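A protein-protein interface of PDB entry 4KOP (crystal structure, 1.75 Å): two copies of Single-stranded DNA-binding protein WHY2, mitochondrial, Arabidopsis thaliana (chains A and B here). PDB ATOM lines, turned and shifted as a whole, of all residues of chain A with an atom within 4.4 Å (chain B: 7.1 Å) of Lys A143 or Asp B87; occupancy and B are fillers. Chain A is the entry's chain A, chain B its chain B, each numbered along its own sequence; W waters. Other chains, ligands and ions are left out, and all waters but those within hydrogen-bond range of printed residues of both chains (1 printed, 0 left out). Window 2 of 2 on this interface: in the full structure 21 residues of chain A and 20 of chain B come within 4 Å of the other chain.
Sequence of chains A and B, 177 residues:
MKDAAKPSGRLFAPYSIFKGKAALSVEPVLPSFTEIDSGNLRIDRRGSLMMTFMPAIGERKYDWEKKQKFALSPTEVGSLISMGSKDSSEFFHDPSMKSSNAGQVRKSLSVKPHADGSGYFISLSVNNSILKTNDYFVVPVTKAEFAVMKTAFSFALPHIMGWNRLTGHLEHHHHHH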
ATOM      1  N   SER A 118      24.997   4.290  28.039  1.00  0.00           N
ATOM      2  CA  SER A 118      24.490   4.826  26.779  1.00  0.00           C
ATOM      3  C   SER A 118      24.842   6.304  26.512  1.00  0.00           C
ATOM      4  O   SER A 118      24.540   6.805  25.441  1.00  0.00           O
ATOM      5  CB  SER A 118      22.998   4.649  26.695  1.00  0.00           C
ATOM      6  OG  SER A 118      22.362   5.431  27.670  1.00  0.00           O
ATOM      7  N   GLY A 119      25.478   6.958  27.471  1.00  0.00           N
ATOM      8  CA  GLY A 119      25.800   8.369  27.399  1.00  0.00           C
ATOM      9  C   GLY A 119      26.043   8.970  28.774  1.00  0.00           C
ATOM     10  O   GLY A 119      26.379   8.252  29.724  1.00  0.00           O
ATOM     11  N   VAL A 141      24.107  13.753  26.790  1.00  0.00           N
ATOM     12  CA  VAL A 141      24.931  13.534  25.625  1.00  0.00           C
ATOM     13  C   VAL A 141      24.966  12.053  25.411  1.00  0.00           C
ATOM     14  O   VAL A 141      25.283  11.311  26.336  1.00  0.00           O
ATOM     15  CB  VAL A 141      26.348  14.101  25.927  1.00  0.00           C
ATOM     16  CG1 VAL A 141      27.293  13.775  24.869  1.00  0.00           C
ATOM     17  CG2 VAL A 141      26.257  15.654  26.100  1.00  0.00           C
ATOM     18  N   THR A 142      24.641  11.611  24.199  1.00  0.00           N
ATOM     19  CA  THR A 142      24.667  10.212  23.861  1.00  0.00           C
ATOM     20  C   THR A 142      26.086   9.725  23.684  1.00  0.00           C
ATOM     21  O   THR A 142      27.041  10.508  23.565  1.00  0.00           O
ATOM     22  CB  THR A 142      23.962   9.931  22.541  1.00  0.00           C
ATOM     23  OG1 THR A 142      24.666  10.599  21.484  1.00  0.00           O
ATOM     24  CG2 THR A 142      22.501  10.395  22.563  1.00  0.00           C
ATOM     25  N   LYS A 143      26.224   8.408  23.644  1.00  0.00           N
ATOM     26  CA  LYS A 143      27.510   7.806  23.381  1.00  0.00           C
ATOM     27  C   LYS A 143      28.102   8.372  22.071  1.00  0.00           C
ATOM     28  O   LYS A 143      29.317   8.658  21.995  1.00  0.00           O
ATOM     29  CB  LYS A 143      27.380   6.286  23.336  1.00  0.00           C
ATOM     30  CG  LYS A 143      28.630   5.574  22.894  1.00  0.00           C
ATOM     31  CD  LYS A 143      28.423   4.049  22.947  1.00  0.00           C
ATOM     32  CE  LYS A 143      29.682   3.302  22.575  1.00  0.00           C
ATOM     33  NZ  LYS A 143      29.440   1.831  22.508  1.00  0.00           N
ATOM     34  N   ALA A 144      27.262   8.528  21.056  1.00  0.00           N
ATOM     35  CA  ALA A 144      27.735   9.046  19.751  1.00  0.00           C
ATOM     36  C   ALA A 144      28.261  10.479  19.881  1.00  0.00           C
ATOM     37  O   ALA A 144      29.323  10.837  19.323  1.00  0.00           O
ATOM     38  CB  ALA A 144      26.616   9.000  18.681  1.00  0.00           C
ATOM     39  N   GLU A 145      27.488  11.319  20.541  1.00  0.00           N
ATOM     40  CA  GLU A 145      27.863  12.718  20.744  1.00  0.00           C
ATOM     41  C   GLU A 145      29.178  12.858  21.549  1.00  0.00           C
ATOM     42  O   GLU A 145      30.036  13.695  21.244  1.00  0.00           O
ATOM     43  CB  GLU A 145      26.714  13.494  21.420  1.00  0.00           C
ATOM     44  CG  GLU A 145      25.501  13.644  20.516  1.00  0.00           C
ATOM     45  CD  GLU A 145      24.208  14.069  21.193  1.00  0.00           C
ATOM     46  OE1 GLU A 145      24.046  13.896  22.433  1.00  0.00           O
ATOM     47  OE2 GLU A 145      23.322  14.571  20.442  1.00  0.00           O
ATOM     48  N   PHE A 146      29.337  12.042  22.572  1.00  0.00           N
ATOM     49  CA  PHE A 146      30.562  12.064  23.361  1.00  0.00           C
ATOM     50  C   PHE A 146      31.763  11.556  22.550  1.00  0.00           C
ATOM     51  O   PHE A 146      32.902  12.042  22.705  1.00  0.00           O
ATOM     52  CB  PHE A 146      30.406  11.269  24.661  1.00  0.00           C
ATOM     53  CG  PHE A 146      31.487  11.574  25.700  1.00  0.00           C
ATOM     54  CD1 PHE A 146      31.593  12.831  26.276  1.00  0.00           C
ATOM     55  CD2 PHE A 146      32.404  10.606  26.061  1.00  0.00           C
ATOM     56  CE1 PHE A 146      32.590  13.119  27.210  1.00  0.00           C
ATOM     57  CE2 PHE A 146      33.398  10.882  26.979  1.00  0.00           C
ATOM     58  CZ  PHE A 146      33.492  12.121  27.561  1.00  0.00           C
ATOM     59  N   ALA A 147      31.519  10.600  21.676  1.00  0.00           N
ATOM     60  CA  ALA A 147      32.552  10.120  20.754  1.00  0.00           C
ATOM     61  C   ALA A 147      33.038  11.266  19.837  1.00  0.00           C
ATOM     62  O   ALA A 147      34.247  11.405  19.566  1.00  0.00           O
ATOM     63  CB  ALA A 147      32.068   8.946  19.950  1.00  0.00           C
ATOM     64  N   THR B  75      27.536  13.757  14.313  1.00  0.00           N
ATOM     65  CA  THR B  75      27.021  12.900  15.367  1.00  0.00           C
ATOM     66  C   THR B  75      26.846  11.430  14.894  1.00  0.00           C
ATOM     67  O   THR B  75      27.247  10.488  15.592  1.00  0.00           O
ATOM     68  CB  THR B  75      25.724  13.481  15.928  1.00  0.00           C
ATOM     69  OG1 THR B  75      25.985  14.770  16.532  1.00  0.00           O
ATOM     70  CG2 THR B  75      25.108  12.532  16.971  1.00  0.00           C
ATOM     71  N   GLY B  78      30.147   9.888  14.745  1.00  0.00           N
ATOM     72  CA  GLY B  78      30.522   9.500  16.093  1.00  0.00           C
ATOM     73  C   GLY B  78      29.950   8.150  16.500  1.00  0.00           C
ATOM     74  O   GLY B  78      30.592   7.351  17.189  1.00  0.00           O
ATOM     75  N   SER B  79      28.726   7.893  16.057  1.00  0.00           N
ATOM     76  CA  SER B  79      28.066   6.630  16.340  1.00  0.00           C
ATOM     77  C   SER B  79      28.878   5.455  15.797  1.00  0.00           C
ATOM     78  O   SER B  79      29.111   4.456  16.487  1.00  0.00           O
ATOM     79  CB  SER B  79      26.668   6.646  15.733  1.00  0.00           C
ATOM     80  OG  SER B  79      25.894   5.642  16.308  1.00  0.00           O
ATOM     81  N   SER B  82      32.440   4.854  17.378  1.00  0.00           N
ATOM     82  CA  SER B  82      32.382   4.346  18.739  1.00  0.00           C
ATOM     83  C   SER B  82      31.861   2.899  18.878  1.00  0.00           C
ATOM     84  O   SER B  82      31.755   2.381  20.008  1.00  0.00           O
ATOM     85  CB  SER B  82      31.621   5.321  19.649  1.00  0.00           C
ATOM     86  OG  SER B  82      30.270   5.465  19.303  1.00  0.00           O
ATOM     87  N   MET B  83      31.554   2.262  17.738  1.00  0.00           N
ATOM     88  CA  MET B  83      31.045   0.885  17.719  1.00  0.00           C
ATOM     89  C   MET B  83      32.133  -0.119  17.974  1.00  0.00           C
ATOM     90  O   MET B  83      33.192  -0.057  17.360  1.00  0.00           O
ATOM     91  CB  MET B  83      30.442   0.565  16.357  1.00  0.00           C
ATOM     92  CG  MET B  83      29.185   1.272  16.110  1.00  0.00           C
ATOM     93  SD  MET B  83      28.458   1.006  14.506  1.00  0.00           S
ATOM     94  CE  MET B  83      28.019  -0.735  14.581  1.00  0.00           C
ATOM     95  N   GLY B  84      31.858  -1.063  18.868  1.00  0.00           N
ATOM     96  CA  GLY B  84      32.701  -2.237  19.022  1.00  0.00           C
ATOM     97  C   GLY B  84      32.142  -3.369  18.170  1.00  0.00           C
ATOM     98  O   GLY B  84      31.098  -3.207  17.534  1.00  0.00           O
ATOM     99  N   SER B  85      32.821  -4.517  18.189  1.00  0.00           N
ATOM    100  CA  SER B  85      32.483  -5.651  17.323  1.00  0.00           C
ATOM    101  C   SER B  85      31.089  -6.216  17.556  1.00  0.00           C
ATOM    102  O   SER B  85      30.560  -6.911  16.695  1.00  0.00           O
ATOM    103  CB  SER B  85      33.515  -6.764  17.493  1.00  0.00           C
ATOM    104  OG  SER B  85      33.540  -7.222  18.826  1.00  0.00           O
ATOM    105  N   LYS B  86      30.490  -5.933  18.705  1.00  0.00           N
ATOM    106  CA  LYS B  86      29.144  -6.426  18.998  1.00  0.00           C
ATOM    107  C   LYS B  86      28.087  -5.335  18.967  1.00  0.00           C
ATOM    108  O   LYS B  86      26.929  -5.587  19.287  1.00  0.00           O
ATOM    109  CB  LYS B  86      29.103  -7.085  20.383  1.00  0.00           C
ATOM    110  CG  LYS B  86      30.131  -8.190  20.581  1.00  0.00           C
ATOM    111  CD  LYS B  86      30.204  -8.599  22.060  1.00  0.00           C
ATOM    112  CE  LYS B  86      29.122  -9.597  22.452  1.00  0.00           C
ATOM    113  NZ  LYS B  86      29.404 -10.962  21.905  1.00  0.00           N
ATOM    114  N   ASP B  87      28.471  -4.120  18.587  1.00  0.00           N
ATOM    115  CA  ASP B  87      27.523  -3.027  18.589  1.00  0.00           C
ATOM    116  C   ASP B  87      26.787  -2.898  17.271  1.00  0.00           C
ATOM    117  O   ASP B  87      27.273  -3.347  16.231  1.00  0.00           O
ATOM    118  CB  ASP B  87      28.249  -1.718  18.925  1.00  0.00           C
ATOM    119  CG  ASP B  87      28.679  -1.650  20.374  1.00  0.00           C
ATOM    120  OD1 ASP B  87      27.826  -1.949  21.236  1.00  0.00           O
ATOM    121  OD2 ASP B  87      29.860  -1.313  20.643  1.00  0.00           O
ATOM    122  N   SER B  88      25.628  -2.241  17.336  1.00  0.00           N
ATOM    123  CA  SER B  88      24.837  -1.874  16.169  1.00  0.00           C
ATOM    124  C   SER B  88      24.600  -0.359  16.108  1.00  0.00           C
ATOM    125  O   SER B  88      24.637   0.329  17.136  1.00  0.00           O
ATOM    126  CB  SER B  88      23.478  -2.558  16.209  1.00  0.00           C
ATOM    127  OG  SER B  88      23.602  -3.925  15.861  1.00  0.00           O
ATOM    128  N   SER B  89      24.340   0.137  14.896  1.00  0.00           N
ATOM    129  CA  SER B  89      23.925   1.523  14.675  1.00  0.00           C
ATOM    130  C   SER B  89      22.792   1.524  13.675  1.00  0.00           C
ATOM    131  O   SER B  89      22.776   0.717  12.762  1.00  0.00           O
ATOM    132  CB  SER B  89      25.072   2.364  14.119  1.00  0.00           C
ATOM    133  OG  SER B  89      25.939   2.801  15.156  1.00  0.00           O
ATOM    134  N   VAL B 111      23.918  -0.637  10.425  1.00  0.00           N
ATOM    135  CA  VAL B 111      25.217  -1.267  10.542  1.00  0.00           C
ATOM    136  C   VAL B 111      25.059  -2.325  11.642  1.00  0.00           C
ATOM    137  O   VAL B 111      24.973  -1.989  12.839  1.00  0.00           O
ATOM    138  CB  VAL B 111      26.326  -0.254  10.937  1.00  0.00           C
ATOM    139  CG1 VAL B 111      27.672  -0.932  10.969  1.00  0.00           C
ATOM    140  CG2 VAL B 111      26.377   0.910   9.954  1.00  0.00           C
ATOM    141  N   LYS B 112      25.021  -3.597  11.241  1.00  0.00           N
ATOM    142  CA  LYS B 112      24.715  -4.702  12.161  1.00  0.00           C
ATOM    143  C   LYS B 112      25.827  -5.740  12.126  1.00  0.00           C
ATOM    144  O   LYS B 112      26.258  -6.112  11.050  1.00  0.00           O
ATOM    145  CB  LYS B 112      23.402  -5.372  11.759  1.00  0.00           C
ATOM    146  CG  LYS B 112      22.157  -4.505  11.934  1.00  0.00           C
ATOM    147  CD  LYS B 112      20.897  -5.373  11.964  1.00  0.00           C
ATOM    148  CE  LYS B 112      19.639  -4.587  12.339  1.00  0.00           C
ATOM    149  NZ  LYS B 112      19.066  -3.816  11.192  1.00  0.00           N
ATOM    150  N   PRO B 113      26.309  -6.165  13.301  1.00  0.00           N
ATOM    151  CA  PRO B 113      27.468  -7.050  13.395  1.00  0.00           C
ATOM    152  C   PRO B 113      27.120  -8.506  13.085  1.00  0.00           C
ATOM    153  O   PRO B 113      26.012  -8.951  13.385  1.00  0.00           O
ATOM    154  CB  PRO B 113      27.888  -6.934  14.862  1.00  0.00           C
ATOM    155  CG  PRO B 113      26.658  -6.590  15.587  1.00  0.00           C
ATOM    156  CD  PRO B 113      25.776  -5.823  14.630  1.00  0.00           C
ATOM    157  N   HIS B 114      28.061  -9.212  12.485  1.00  0.00           N
ATOM    158  CA  HIS B 114      27.995 -10.684  12.408  1.00  0.00           C
ATOM    159  C   HIS B 114      28.253 -11.230  13.803  1.00  0.00           C
ATOM    160  O   HIS B 114      29.060 -10.674  14.562  1.00  0.00           O
ATOM    161  CB  HIS B 114      29.076 -11.226  11.471  1.00  0.00           C
ATOM    162  CG  HIS B 114      29.048 -10.642  10.092  1.00  0.00           C
ATOM    163  ND1 HIS B 114      27.883 -10.381   9.413  1.00  0.00           N
ATOM    164  CD2 HIS B 114      30.054 -10.262   9.269  1.00  0.00           C
ATOM    165  CE1 HIS B 114      28.167  -9.871   8.230  1.00  0.00           C
ATOM    166  NE2 HIS B 114      29.479  -9.802   8.110  1.00  0.00           N
ATOM    167  N   GLY B 119      32.836  -8.816  11.157  1.00  0.00           N
ATOM    168  CA  GLY B 119      32.432  -7.682  10.341  1.00  0.00           C
ATOM    169  C   GLY B 119      30.988  -7.306  10.575  1.00  0.00           C
ATOM    170  O   GLY B 119      30.433  -7.591  11.630  1.00  0.00           O
ATOM    171  N   TYR B 120      30.396  -6.664   9.571  1.00  0.00           N
ATOM    172  CA  TYR B 120      29.059  -6.073   9.663  1.00  0.00           C
ATOM    173  C   TYR B 120      28.346  -6.170   8.318  1.00  0.00           C
ATOM    174  O   TYR B 120      28.979  -6.320   7.267  1.00  0.00           O
ATOM    175  CB  TYR B 120      29.146  -4.580  10.013  1.00  0.00           C
ATOM    176  CG  TYR B 120      29.911  -4.263  11.262  1.00  0.00           C
ATOM    177  CD1 TYR B 120      31.300  -4.205  11.253  1.00  0.00           C
ATOM    178  CD2 TYR B 120      29.249  -4.008  12.445  1.00  0.00           C
ATOM    179  CE1 TYR B 120      32.000  -3.924  12.405  1.00  0.00           C
ATOM    180  CE2 TYR B 120      29.930  -3.723  13.587  1.00  0.00           C
ATOM    181  CZ  TYR B 120      31.302  -3.674  13.558  1.00  0.00           C
ATOM    182  OH  TYR B 120      31.966  -3.361  14.692  1.00  0.00           O
HETATM  183  O   HOH W   1      23.711  15.700  18.008  1.00  0.00           O
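The side-chain amino group (NZ) of Lys A143 sits close to the backbone carbonyl oxygen (O) of Ser B82, at 3.5 Å. The side-chain carboxylate (OD2) of Asp B87 is in salt-bridge range of the side-chain amino group (NZ) of Lys A143, 3.7 Å away.
CB of Ala A144 touches O of Thr B75, 3.5 Å away. CA of Gly B78 touches O of Ala A144, at 3.7 Å. Ser B79 touches Ala A144 (N to CB, 3.5 Å). CG2 of Thr B75 touches CG of Glu A145, at 3.7 Å. O of Gly B78 touches CB of Ala A147 (3.5 Å). CB of Ala A147 touches CB of Ser B82 (3.7 Å).
1 position is printed for both chains. Of the 8 pairs that touch across the chains among the printed residues, none has its exchanged pair printed and touching as well.
Of the 17 printed residues of chain B, 5 touch a printed residue of chain A. Printed residues of chain B that touch a printed residue of chain A: Thr B75, Gly B78, Ser B79, Ser B82 and Asp B87. Among the printed residues, 8 pairs touch across the chains.
N of Lys A143 is in hydrogen-bond range of O of Ser A118, 2.9 Å away. The side-chain hydroxyl (OG) of Ser B79 lies within hydrogen-bond range of the side-chain hydroxyl (OG) of Ser B89, at 3.1 Å. The backbone NH (N) of Thr A142 is in hydrogen-bond range of the side-chain carboxylate (OE1) of Glu A145 (2.9 Å). The backbone carbonyl oxygen (O) of Ser B79 sits at hydrogen-bond distance from the side-chain hydroxyl (OG) of Ser B82, 3.2 Å away. The backbone NH of Gly B84 lies within hydrogen-bond range of the side-chain carboxylate of Asp B87 (2.7 Å). The backbone carbonyl oxygen of Gly B78 lies within hydrogen-bond range of the side-chain hydroxyl of Ser B82.
Water W1 lies within hydrogen-bond range of the side-chain carboxylate of Glu A145 (2.7 Å) and the side-chain hydroxyl of Thr B75 (2.9 Å).
Of chain B, only Ser B82 and Asp B87 come within 4 Å of Lys A143. Printed residues of chain A within 4 Å of Ser B79: Ala A144. Of the printed residues of chain B, Ala A144 touches Thr B75, Gly B78 and Ser B79. Tyr B120 touches none of the printed residues of chain A.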
